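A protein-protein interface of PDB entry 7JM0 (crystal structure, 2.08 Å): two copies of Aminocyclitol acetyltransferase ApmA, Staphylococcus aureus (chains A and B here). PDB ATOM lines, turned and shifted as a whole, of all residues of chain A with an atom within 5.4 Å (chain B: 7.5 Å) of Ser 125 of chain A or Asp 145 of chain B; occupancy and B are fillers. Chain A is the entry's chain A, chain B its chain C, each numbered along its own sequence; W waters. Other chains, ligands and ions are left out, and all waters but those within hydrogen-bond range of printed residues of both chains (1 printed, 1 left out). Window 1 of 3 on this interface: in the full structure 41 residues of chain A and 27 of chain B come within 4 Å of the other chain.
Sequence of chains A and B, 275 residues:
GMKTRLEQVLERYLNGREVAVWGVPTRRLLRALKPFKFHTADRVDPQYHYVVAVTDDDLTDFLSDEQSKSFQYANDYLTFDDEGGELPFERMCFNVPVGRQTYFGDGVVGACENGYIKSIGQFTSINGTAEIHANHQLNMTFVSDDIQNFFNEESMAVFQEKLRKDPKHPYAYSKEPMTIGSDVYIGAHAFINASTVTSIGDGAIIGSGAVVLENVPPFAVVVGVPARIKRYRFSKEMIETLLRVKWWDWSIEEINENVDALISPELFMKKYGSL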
ATOM      1  N   THR A 102      -4.337  11.901   7.098  1.00  0.00           N
ATOM      2  CA  THR A 102      -3.261  12.382   7.950  1.00  0.00           C
ATOM      3  C   THR A 102      -2.000  11.584   7.654  1.00  0.00           C
ATOM      4  O   THR A 102      -2.049  10.352   7.566  1.00  0.00           O
ATOM      5  CB  THR A 102      -3.641  12.262   9.426  1.00  0.00           C
ATOM      6  OG1 THR A 102      -4.673  13.208   9.725  1.00  0.00           O
ATOM      7  CG2 THR A 102      -2.440  12.526  10.325  1.00  0.00           C
ATOM      8  N   TYR A 103      -0.879  12.281   7.485  1.00  0.00           N
ATOM      9  CA  TYR A 103       0.378  11.623   7.171  1.00  0.00           C
ATOM     10  C   TYR A 103       1.500  12.172   8.038  1.00  0.00           C
ATOM     11  O   TYR A 103       1.413  13.272   8.591  1.00  0.00           O
ATOM     12  CB  TYR A 103       0.741  11.770   5.687  1.00  0.00           C
ATOM     13  CG  TYR A 103       0.847  13.199   5.194  1.00  0.00           C
ATOM     14  CD1 TYR A 103       2.049  13.893   5.264  1.00  0.00           C
ATOM     15  CD2 TYR A 103      -0.250  13.845   4.642  1.00  0.00           C
ATOM     16  CE1 TYR A 103       2.152  15.197   4.803  1.00  0.00           C
ATOM     17  CE2 TYR A 103      -0.158  15.145   4.178  1.00  0.00           C
ATOM     18  CZ  TYR A 103       1.045  15.815   4.261  1.00  0.00           C
ATOM     19  OH  TYR A 103       1.138  17.109   3.800  1.00  0.00           O
ATOM     20  N   PHE A 123      -6.912  15.072   8.797  1.00  0.00           N
ATOM     21  CA  PHE A 123      -6.420  16.084   7.857  1.00  0.00           C
ATOM     22  C   PHE A 123      -5.212  16.828   8.420  1.00  0.00           C
ATOM     23  O   PHE A 123      -5.090  18.048   8.291  1.00  0.00           O
ATOM     24  CB  PHE A 123      -7.537  17.057   7.467  1.00  0.00           C
ATOM     25  CG  PHE A 123      -8.795  16.370   7.021  1.00  0.00           C
ATOM     26  CD1 PHE A 123      -8.860  15.764   5.778  1.00  0.00           C
ATOM     27  CD2 PHE A 123      -9.906  16.319   7.847  1.00  0.00           C
ATOM     28  CE1 PHE A 123     -10.012  15.119   5.362  1.00  0.00           C
ATOM     29  CE2 PHE A 123     -11.064  15.676   7.437  1.00  0.00           C
ATOM     30  CZ  PHE A 123     -11.114  15.075   6.193  1.00  0.00           C
ATOM     31  N   THR A 124      -4.307  16.084   9.042  1.00  0.00           N
ATOM     32  CA  THR A 124      -3.115  16.642   9.658  1.00  0.00           C
ATOM     33  C   THR A 124      -1.897  16.287   8.820  1.00  0.00           C
ATOM     34  O   THR A 124      -1.761  15.153   8.351  1.00  0.00           O
ATOM     35  CB  THR A 124      -2.970  16.138  11.096  1.00  0.00           C
ATOM     36  OG1 THR A 124      -3.890  16.858  11.922  1.00  0.00           O
ATOM     37  CG2 THR A 124      -1.547  16.339  11.630  1.00  0.00           C
ATOM     38  N   SER A 125      -1.025  17.271   8.614  1.00  0.00           N
ATOM     39  CA  SER A 125       0.105  17.156   7.698  1.00  0.00           C
ATOM     40  C   SER A 125       1.389  17.368   8.486  1.00  0.00           C
ATOM     41  O   SER A 125       1.636  18.469   8.994  1.00  0.00           O
ATOM     42  CB  SER A 125      -0.016  18.170   6.565  1.00  0.00           C
ATOM     43  OG  SER A 125      -1.323  18.161   6.017  1.00  0.00           O
ATOM     44  N   ILE A 126       2.203  16.325   8.590  1.00  0.00           N
ATOM     45  CA  ILE A 126       3.457  16.371   9.329  1.00  0.00           C
ATOM     46  C   ILE A 126       4.577  16.037   8.357  1.00  0.00           C
ATOM     47  O   ILE A 126       4.620  14.925   7.812  1.00  0.00           O
ATOM     48  CB  ILE A 126       3.455  15.408  10.527  1.00  0.00           C
ATOM     49  CG1 ILE A 126       2.233  15.672  11.412  1.00  0.00           C
ATOM     50  CG2 ILE A 126       4.747  15.542  11.322  1.00  0.00           C
ATOM     51  CD1 ILE A 126       2.125  14.755  12.608  1.00  0.00           C
ATOM     52  N   ASN A 127       5.471  17.000   8.132  1.00  0.00           N
ATOM     53  CA  ASN A 127       6.562  16.811   7.188  1.00  0.00           C
ATOM     54  C   ASN A 127       7.413  15.610   7.583  1.00  0.00           C
ATOM     55  O   ASN A 127       7.564  15.286   8.766  1.00  0.00           O
ATOM     56  CB  ASN A 127       7.425  18.071   7.111  1.00  0.00           C
ATOM     57  CG  ASN A 127       8.387  18.048   5.938  1.00  0.00           C
ATOM     58  OD1 ASN A 127       9.454  17.439   6.008  1.00  0.00           O
ATOM     59  ND2 ASN A 127       8.010  18.711   4.848  1.00  0.00           N
ATOM     60  N   VAL A 184      -3.789  20.008  11.605  1.00  0.00           N
ATOM     61  CA  VAL A 184      -2.500  20.472  12.103  1.00  0.00           C
ATOM     62  C   VAL A 184      -1.480  20.393  10.975  1.00  0.00           C
ATOM     63  O   VAL A 184      -1.537  19.505  10.117  1.00  0.00           O
ATOM     64  CB  VAL A 184      -2.061  19.642  13.329  1.00  0.00           C
ATOM     65  CG1 VAL A 184      -0.622  19.959  13.730  1.00  0.00           C
ATOM     66  CG2 VAL A 184      -3.005  19.891  14.500  1.00  0.00           C
ATOM     67  N   TYR A 185      -0.546  21.339  10.960  1.00  0.00           N
ATOM     68  CA  TYR A 185       0.570  21.317  10.025  1.00  0.00           C
ATOM     69  C   TYR A 185       1.866  21.460  10.802  1.00  0.00           C
ATOM     70  O   TYR A 185       2.021  22.397  11.592  1.00  0.00           O
ATOM     71  CB  TYR A 185       0.463  22.434   8.981  1.00  0.00           C
ATOM     72  CG  TYR A 185       1.591  22.408   7.974  1.00  0.00           C
ATOM     73  CD1 TYR A 185       1.566  21.532   6.897  1.00  0.00           C
ATOM     74  CD2 TYR A 185       2.692  23.244   8.111  1.00  0.00           C
ATOM     75  CE1 TYR A 185       2.596  21.500   5.977  1.00  0.00           C
ATOM     76  CE2 TYR A 185       3.729  23.217   7.196  1.00  0.00           C
ATOM     77  CZ  TYR A 185       3.674  22.343   6.131  1.00  0.00           C
ATOM     78  OH  TYR A 185       4.702  22.312   5.214  1.00  0.00           O
ATOM     79  N   ILE A 186       2.794  20.534  10.573  1.00  0.00           N
ATOM     80  CA  ILE A 186       4.116  20.564  11.184  1.00  0.00           C
ATOM     81  C   ILE A 186       5.146  20.586  10.063  1.00  0.00           C
ATOM     82  O   ILE A 186       5.131  19.716   9.184  1.00  0.00           O
ATOM     83  CB  ILE A 186       4.336  19.364  12.122  1.00  0.00           C
ATOM     84  CG1 ILE A 186       3.269  19.356  13.220  1.00  0.00           C
ATOM     85  CG2 ILE A 186       5.730  19.417  12.729  1.00  0.00           C
ATOM     86  CD1 ILE A 186       3.325  18.148  14.132  1.00  0.00           C
ATOM     87  N   HIS B 133      11.111  22.771   0.197  1.00  0.00           N
ATOM     88  CA  HIS B 133       9.685  22.483   0.189  1.00  0.00           C
ATOM     89  C   HIS B 133       8.913  23.793   0.224  1.00  0.00           C
ATOM     90  O   HIS B 133       9.424  24.825   0.662  1.00  0.00           O
ATOM     91  CB  HIS B 133       9.299  21.574   1.371  1.00  0.00           C
ATOM     92  CG  HIS B 133       8.326  20.485   1.024  1.00  0.00           C
ATOM     93  ND1 HIS B 133       8.621  19.499   0.103  1.00  0.00           N
ATOM     94  CD2 HIS B 133       7.079  20.214   1.497  1.00  0.00           C
ATOM     95  CE1 HIS B 133       7.581  18.688   0.011  1.00  0.00           C
ATOM     96  NE2 HIS B 133       6.635  19.094   0.845  1.00  0.00           N
ATOM     97  N   HIS B 136       1.971  25.054   2.494  1.00  0.00           N
ATOM     98  CA  HIS B 136       0.553  24.875   2.239  1.00  0.00           C
ATOM     99  C   HIS B 136      -0.130  26.238   2.188  1.00  0.00           C
ATOM    100  O   HIS B 136       0.443  27.266   2.564  1.00  0.00           O
ATOM    101  CB  HIS B 136      -0.092  24.012   3.325  1.00  0.00           C
ATOM    102  CG  HIS B 136       0.337  22.578   3.303  1.00  0.00           C
ATOM    103  ND1 HIS B 136      -0.369  21.583   3.945  1.00  0.00           N
ATOM    104  CD2 HIS B 136       1.397  21.970   2.719  1.00  0.00           C
ATOM    105  CE1 HIS B 136       0.239  20.424   3.761  1.00  0.00           C
ATOM    106  NE2 HIS B 136       1.314  20.630   3.021  1.00  0.00           N
ATOM    107  N   GLN B 137      -1.373  26.246   1.711  1.00  0.00           N
ATOM    108  CA  GLN B 137      -2.170  27.462   1.787  1.00  0.00           C
ATOM    109  C   GLN B 137      -2.366  27.847   3.250  1.00  0.00           C
ATOM    110  O   GLN B 137      -2.605  26.994   4.111  1.00  0.00           O
ATOM    111  CB  GLN B 137      -3.517  27.273   1.079  1.00  0.00           C
ATOM    112  CG  GLN B 137      -4.552  26.449   1.840  1.00  0.00           C
ATOM    113  CD  GLN B 137      -4.244  24.967   1.846  1.00  0.00           C
ATOM    114  OE1 GLN B 137      -3.414  24.486   1.071  1.00  0.00           O
ATOM    115  NE2 GLN B 137      -4.921  24.228   2.719  1.00  0.00           N
ATOM    116  N   PHE B 142      -8.872  25.621   6.214  1.00  0.00           N
ATOM    117  CA  PHE B 142      -8.055  24.446   6.461  1.00  0.00           C
ATOM    118  C   PHE B 142      -6.636  24.687   5.970  1.00  0.00           C
ATOM    119  O   PHE B 142      -6.402  25.474   5.047  1.00  0.00           O
ATOM    120  CB  PHE B 142      -8.632  23.196   5.771  1.00  0.00           C
ATOM    121  CG  PHE B 142      -8.719  23.313   4.277  1.00  0.00           C
ATOM    122  CD1 PHE B 142      -9.807  23.931   3.678  1.00  0.00           C
ATOM    123  CD2 PHE B 142      -7.719  22.799   3.468  1.00  0.00           C
ATOM    124  CE1 PHE B 142      -9.893  24.040   2.298  1.00  0.00           C
ATOM    125  CE2 PHE B 142      -7.799  22.904   2.088  1.00  0.00           C
ATOM    126  CZ  PHE B 142      -8.887  23.525   1.504  1.00  0.00           C
ATOM    127  N   VAL B 143      -5.691  23.992   6.597  1.00  0.00           N
ATOM    128  CA  VAL B 143      -4.294  24.011   6.179  1.00  0.00           C
ATOM    129  C   VAL B 143      -3.869  22.701   5.532  1.00  0.00           C
ATOM    130  O   VAL B 143      -2.797  22.653   4.900  1.00  0.00           O
ATOM    131  CB  VAL B 143      -3.361  24.355   7.362  1.00  0.00           C
ATOM    132  CG1 VAL B 143      -3.192  23.149   8.281  1.00  0.00           C
ATOM    133  CG2 VAL B 143      -2.013  24.874   6.870  1.00  0.00           C
ATOM    134  N   SER B 144      -4.677  21.648   5.644  1.00  0.00           N
ATOM    135  CA  SER B 144      -4.348  20.359   5.054  1.00  0.00           C
ATOM    136  C   SER B 144      -4.277  20.451   3.535  1.00  0.00           C
ATOM    137  O   SER B 144      -4.992  21.229   2.900  1.00  0.00           O
ATOM    138  CB  SER B 144      -5.392  19.316   5.454  1.00  0.00           C
ATOM    139  OG  SER B 144      -5.400  18.222   4.556  1.00  0.00           O
ATOM    140  N   ASP B 145      -3.400  19.639   2.952  1.00  0.00           N
ATOM    141  CA  ASP B 145      -3.410  19.421   1.512  1.00  0.00           C
ATOM    142  C   ASP B 145      -4.161  18.155   1.119  1.00  0.00           C
ATOM    143  O   ASP B 145      -4.925  18.173   0.151  1.00  0.00           O
ATOM    144  CB  ASP B 145      -1.979  19.373   0.960  1.00  0.00           C
ATOM    145  CG  ASP B 145      -1.114  18.327   1.639  1.00  0.00           C
ATOM    146  OD1 ASP B 145      -1.441  17.915   2.771  1.00  0.00           O
ATOM    147  OD2 ASP B 145      -0.089  17.929   1.044  1.00  0.00           O
ATOM    148  N   ASP B 146      -3.995  17.066   1.872  1.00  0.00           N
ATOM    149  CA  ASP B 146      -4.583  15.788   1.483  1.00  0.00           C
ATOM    150  C   ASP B 146      -6.096  15.743   1.653  1.00  0.00           C
ATOM    151  O   ASP B 146      -6.715  14.751   1.252  1.00  0.00           O
ATOM    152  CB  ASP B 146      -3.933  14.652   2.272  1.00  0.00           C
ATOM    153  CG  ASP B 146      -2.600  14.239   1.687  1.00  0.00           C
ATOM    154  OD1 ASP B 146      -2.131  14.919   0.748  1.00  0.00           O
ATOM    155  OD2 ASP B 146      -2.030  13.232   2.150  1.00  0.00           O
ATOM    156  N   ILE B 147      -6.703  16.782   2.231  1.00  0.00           N
ATOM    157  CA  ILE B 147      -8.157  16.901   2.200  1.00  0.00           C
ATOM    158  C   ILE B 147      -8.654  16.937   0.759  1.00  0.00           C
ATOM    159  O   ILE B 147      -9.778  16.507   0.466  1.00  0.00           O
ATOM    160  CB  ILE B 147      -8.600  18.148   2.991  1.00  0.00           C
ATOM    161  CG1 ILE B 147     -10.126  18.263   3.027  1.00  0.00           C
ATOM    162  CG2 ILE B 147      -7.976  19.407   2.400  1.00  0.00           C
ATOM    163  CD1 ILE B 147     -10.627  19.511   3.723  1.00  0.00           C
ATOM    164  N   GLN B 148      -7.818  17.419  -0.167  1.00  0.00           N
ATOM    165  CA  GLN B 148      -8.198  17.483  -1.573  1.00  0.00           C
ATOM    166  C   GLN B 148      -8.436  16.103  -2.174  1.00  0.00           C
ATOM    167  O   GLN B 148      -9.132  15.994  -3.189  1.00  0.00           O
ATOM    168  CB  GLN B 148      -7.126  18.224  -2.377  1.00  0.00           C
ATOM    169  CG  GLN B 148      -5.894  17.393  -2.702  1.00  0.00           C
ATOM    170  CD  GLN B 148      -4.773  18.226  -3.294  1.00  0.00           C
ATOM    171  OE1 GLN B 148      -5.009  19.294  -3.857  1.00  0.00           O
ATOM    172  NE2 GLN B 148      -3.543  17.742  -3.164  1.00  0.00           N
ATOM    173  N   ASN B 149      -7.880  15.047  -1.575  1.00  0.00           N
ATOM    174  CA  ASN B 149      -8.180  13.697  -2.038  1.00  0.00           C
ATOM    175  C   ASN B 149      -9.660  13.366  -1.896  1.00  0.00           C
ATOM    176  O   ASN B 149     -10.139  12.433  -2.549  1.00  0.00           O
ATOM    177  CB  ASN B 149      -7.331  12.676  -1.277  1.00  0.00           C
ATOM    178  CG  ASN B 149      -5.840  12.870  -1.509  1.00  0.00           C
ATOM    179  OD1 ASN B 149      -5.423  13.317  -2.576  1.00  0.00           O
ATOM    180  ND2 ASN B 149      -5.032  12.535  -0.508  1.00  0.00           N
ATOM    181  N   PHE B 150     -10.391  14.105  -1.063  1.00  0.00           N
ATOM    182  CA  PHE B 150     -11.833  13.943  -0.934  1.00  0.00           C
ATOM    183  C   PHE B 150     -12.626  14.889  -1.829  1.00  0.00           C
ATOM    184  O   PHE B 150     -13.856  14.784  -1.874  1.00  0.00           O
ATOM    185  CB  PHE B 150     -12.261  14.147   0.524  1.00  0.00           C
ATOM    186  CG  PHE B 150     -11.938  12.983   1.422  1.00  0.00           C
ATOM    187  CD1 PHE B 150     -11.726  11.719   0.893  1.00  0.00           C
ATOM    188  CD2 PHE B 150     -11.855  13.154   2.795  1.00  0.00           C
ATOM    189  CE1 PHE B 150     -11.434  10.647   1.716  1.00  0.00           C
ATOM    190  CE2 PHE B 150     -11.564  12.087   3.625  1.00  0.00           C
ATOM    191  CZ  PHE B 150     -11.353  10.832   3.084  1.00  0.00           C
ATOM    192  N   PHE B 151     -11.963  15.805  -2.535  1.00  0.00           N
ATOM    193  CA  PHE B 151     -12.656  16.753  -3.397  1.00  0.00           C
ATOM    194  C   PHE B 151     -13.027  16.084  -4.716  1.00  0.00           C
ATOM    195  O   PHE B 151     -12.183  15.450  -5.356  1.00  0.00           O
ATOM    196  CB  PHE B 151     -11.779  17.978  -3.670  1.00  0.00           C
ATOM    197  CG  PHE B 151     -11.616  18.898  -2.489  1.00  0.00           C
ATOM    198  CD1 PHE B 151     -12.482  18.834  -1.408  1.00  0.00           C
ATOM    199  CD2 PHE B 151     -10.596  19.838  -2.467  1.00  0.00           C
ATOM    200  CE1 PHE B 151     -12.327  19.687  -0.322  1.00  0.00           C
ATOM    201  CE2 PHE B 151     -10.435  20.689  -1.388  1.00  0.00           C
ATOM    202  CZ  PHE B 151     -11.301  20.614  -0.314  1.00  0.00           C
ATOM    203  N   MET B 156     -12.479  20.366  -6.470  1.00  0.00           N
ATOM    204  CA  MET B 156     -11.049  20.494  -6.733  1.00  0.00           C
ATOM    205  C   MET B 156     -10.762  21.678  -7.648  1.00  0.00           C
ATOM    206  O   MET B 156      -9.801  22.422  -7.424  1.00  0.00           O
ATOM    207  CB  MET B 156     -10.502  19.206  -7.347  1.00  0.00           C
ATOM    208  CG  MET B 156      -9.029  19.303  -7.727  1.00  0.00           C
ATOM    209  SD  MET B 156      -7.952  19.359  -6.276  1.00  0.00           S
ATOM    210  CE  MET B 156      -7.868  17.624  -5.866  1.00  0.00           C
ATOM    211  N   PHE B 159     -10.870  24.710  -5.624  1.00  0.00           N
ATOM    212  CA  PHE B 159      -9.676  24.748  -4.787  1.00  0.00           C
ATOM    213  C   PHE B 159      -8.444  25.145  -5.597  1.00  0.00           C
ATOM    214  O   PHE B 159      -7.662  26.004  -5.176  1.00  0.00           O
ATOM    215  CB  PHE B 159      -9.474  23.387  -4.122  1.00  0.00           C
ATOM    216  CG  PHE B 159      -8.275  23.315  -3.219  1.00  0.00           C
ATOM    217  CD1 PHE B 159      -8.090  24.248  -2.210  1.00  0.00           C
ATOM    218  CD2 PHE B 159      -7.348  22.295  -3.361  1.00  0.00           C
ATOM    219  CE1 PHE B 159      -6.988  24.174  -1.370  1.00  0.00           C
ATOM    220  CE2 PHE B 159      -6.248  22.214  -2.525  1.00  0.00           C
ATOM    221  CZ  PHE B 159      -6.066  23.156  -1.528  1.00  0.00           C
ATOM    222  N   TYR B 171       2.330  25.834  -2.416  1.00  0.00           N
ATOM    223  CA  TYR B 171       2.811  24.781  -3.306  1.00  0.00           C
ATOM    224  C   TYR B 171       3.580  25.347  -4.496  1.00  0.00           C
ATOM    225  O   TYR B 171       3.676  24.698  -5.544  1.00  0.00           O
ATOM    226  CB  TYR B 171       1.656  23.883  -3.773  1.00  0.00           C
ATOM    227  CG  TYR B 171       0.735  23.491  -2.637  1.00  0.00           C
ATOM    228  CD1 TYR B 171       1.101  22.501  -1.732  1.00  0.00           C
ATOM    229  CD2 TYR B 171      -0.486  24.126  -2.453  1.00  0.00           C
ATOM    230  CE1 TYR B 171       0.270  22.147  -0.678  1.00  0.00           C
ATOM    231  CE2 TYR B 171      -1.324  23.780  -1.405  1.00  0.00           C
ATOM    232  CZ  TYR B 171      -0.938  22.790  -0.521  1.00  0.00           C
ATOM    233  OH  TYR B 171      -1.764  22.442   0.523  1.00  0.00           O
HETATM  234  O   HOH W   1      -3.474  16.571   5.415  1.00  0.00           O
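Thr 124 of chain A touches none of the printed residues of chain B.
Ser 125 of chain A touches just these residues of chain B: His 136 (3.6 Å), Ser 144 (3.9 Å) and Asp 145 (3.3 Å).
Printed residues of chain B within 4 Å of Tyr 185 of chain A: His 136 (3.3 Å) and Val 143 (3.8 Å).
Of the printed residues of chain A, Val 143 of chain B touches Tyr 185.
Of chain A, only Tyr 103 (2.9 Å) and Ser 125 (3.3 Å) come within 4 Å of Asp 145 of chain B.
Printed residues of chain A within 4 Å of Asp 146 of chain B: Tyr 103 (3.1 Å).
Printed residues of chain A within 4 Å of Ile 147 of chain B: Phe 123.
Of the printed residues of chain A, Phe 150 of chain B touches Phe 123.
The nearest residue of chain B that does not touch Ser 125 of chain A is Val 143 of chain B (4.9 Å).
The nearest printed residue of chain A that does not touch His 136 of chain B is Val 184 of chain A (6.6 Å).
Of the 16 printed residues of chain B, 8 touch a printed residue of chain A.
Printed residues of chain B that touch a printed residue of chain A: His 133, His 136, Val 143, Ser 144, Asp 145, Asp 146, Ile 147 and Phe 150.
Hydrophobic or aromatic side chains of chain B that line the printed part of chain A: His 133, His 136, Val 143, Ile 147 and Phe 150.
Of the 10 printed residues of chain A, 5 touch a printed residue of chain B.
Printed residues of chain A that touch a printed residue of chain B: Tyr 103, Phe 123, Ser 125, Asn 127 and Tyr 185.
Hydrophobic or aromatic side chains of chain A that line the printed part of chain B: Tyr 103, Phe 123 and Tyr 185.
Among the printed residues, 12 pairs touch across the chains.
Among the printed residues, no Asp or Glu carboxylate lies within 4 Å of a Lys or Arg side-chain nitrogen of the other chain.
No position is printed for both chains.
N of Asn 127 of chain A lies within hydrogen-bond range of O of Ile 186 of chain A (2.9 Å).
OG of Ser 144 of chain B sits at hydrogen-bond distance from N of Ile 147 of chain B.
O of Tyr 103 of chain A lies within hydrogen-bond range of N of Ile 126 of chain A, at 3.2 Å.
The backbone carbonyl oxygen (O) of Ser 125 of chain A is in hydrogen-bond range of the backbone NH (N) of Ile 186 of chain A.
The side-chain amide nitrogen (ND2) of Asn 149 of chain B lies within hydrogen-bond range of the backbone carbonyl oxygen (O) of Asp 146 of chain B (3.3 Å).
The side-chain hydroxyl (OH) of Tyr 103 of chain A sits close to the side-chain hydroxyl (OG) of Ser 125 of chain A.
Among the printed residues, pairs that only touch across the chains: Tyr 103 of chain A with His 136 of chain B (3.4 Å), Tyr 103 of chain A with Asp 146 of chain B (3.1 Å), Phe 123 of chain A with Ser 144 of chain B (3.1 Å), Phe 123 of chain A with Ile 147 of chain B (3.7 Å), Phe 123 of chain A with Phe 150 of chain B (3.7 Å), Ser 125 of chain A with His 136 of chain B (3.6 Å), Ser 125 of chain A with Ser 144 of chain B (3.9 Å), Asn 127 of chain A with His 133 of chain B (3.8 Å), Tyr 185 of chain A with His 136 of chain B (3.3 Å) and Tyr 185 of chain A with Val 143 of chain B (3.8 Å).
OH of Tyr 103 of chain A is in hydrogen-bond range of OD1 of Asp 145 of chain B (2.9 Å).
OG of Ser 125 of chain A lies within hydrogen-bond range of OD1 of Asp 145 of chain B, at 3.3 Å.
Water W1 lies within hydrogen-bond range of the side-chain hydroxyl (OG) of Ser 144 of chain B (2.7 Å) and the side-chain hydroxyl (OG) of Ser 125 of chain A (2.7 Å).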
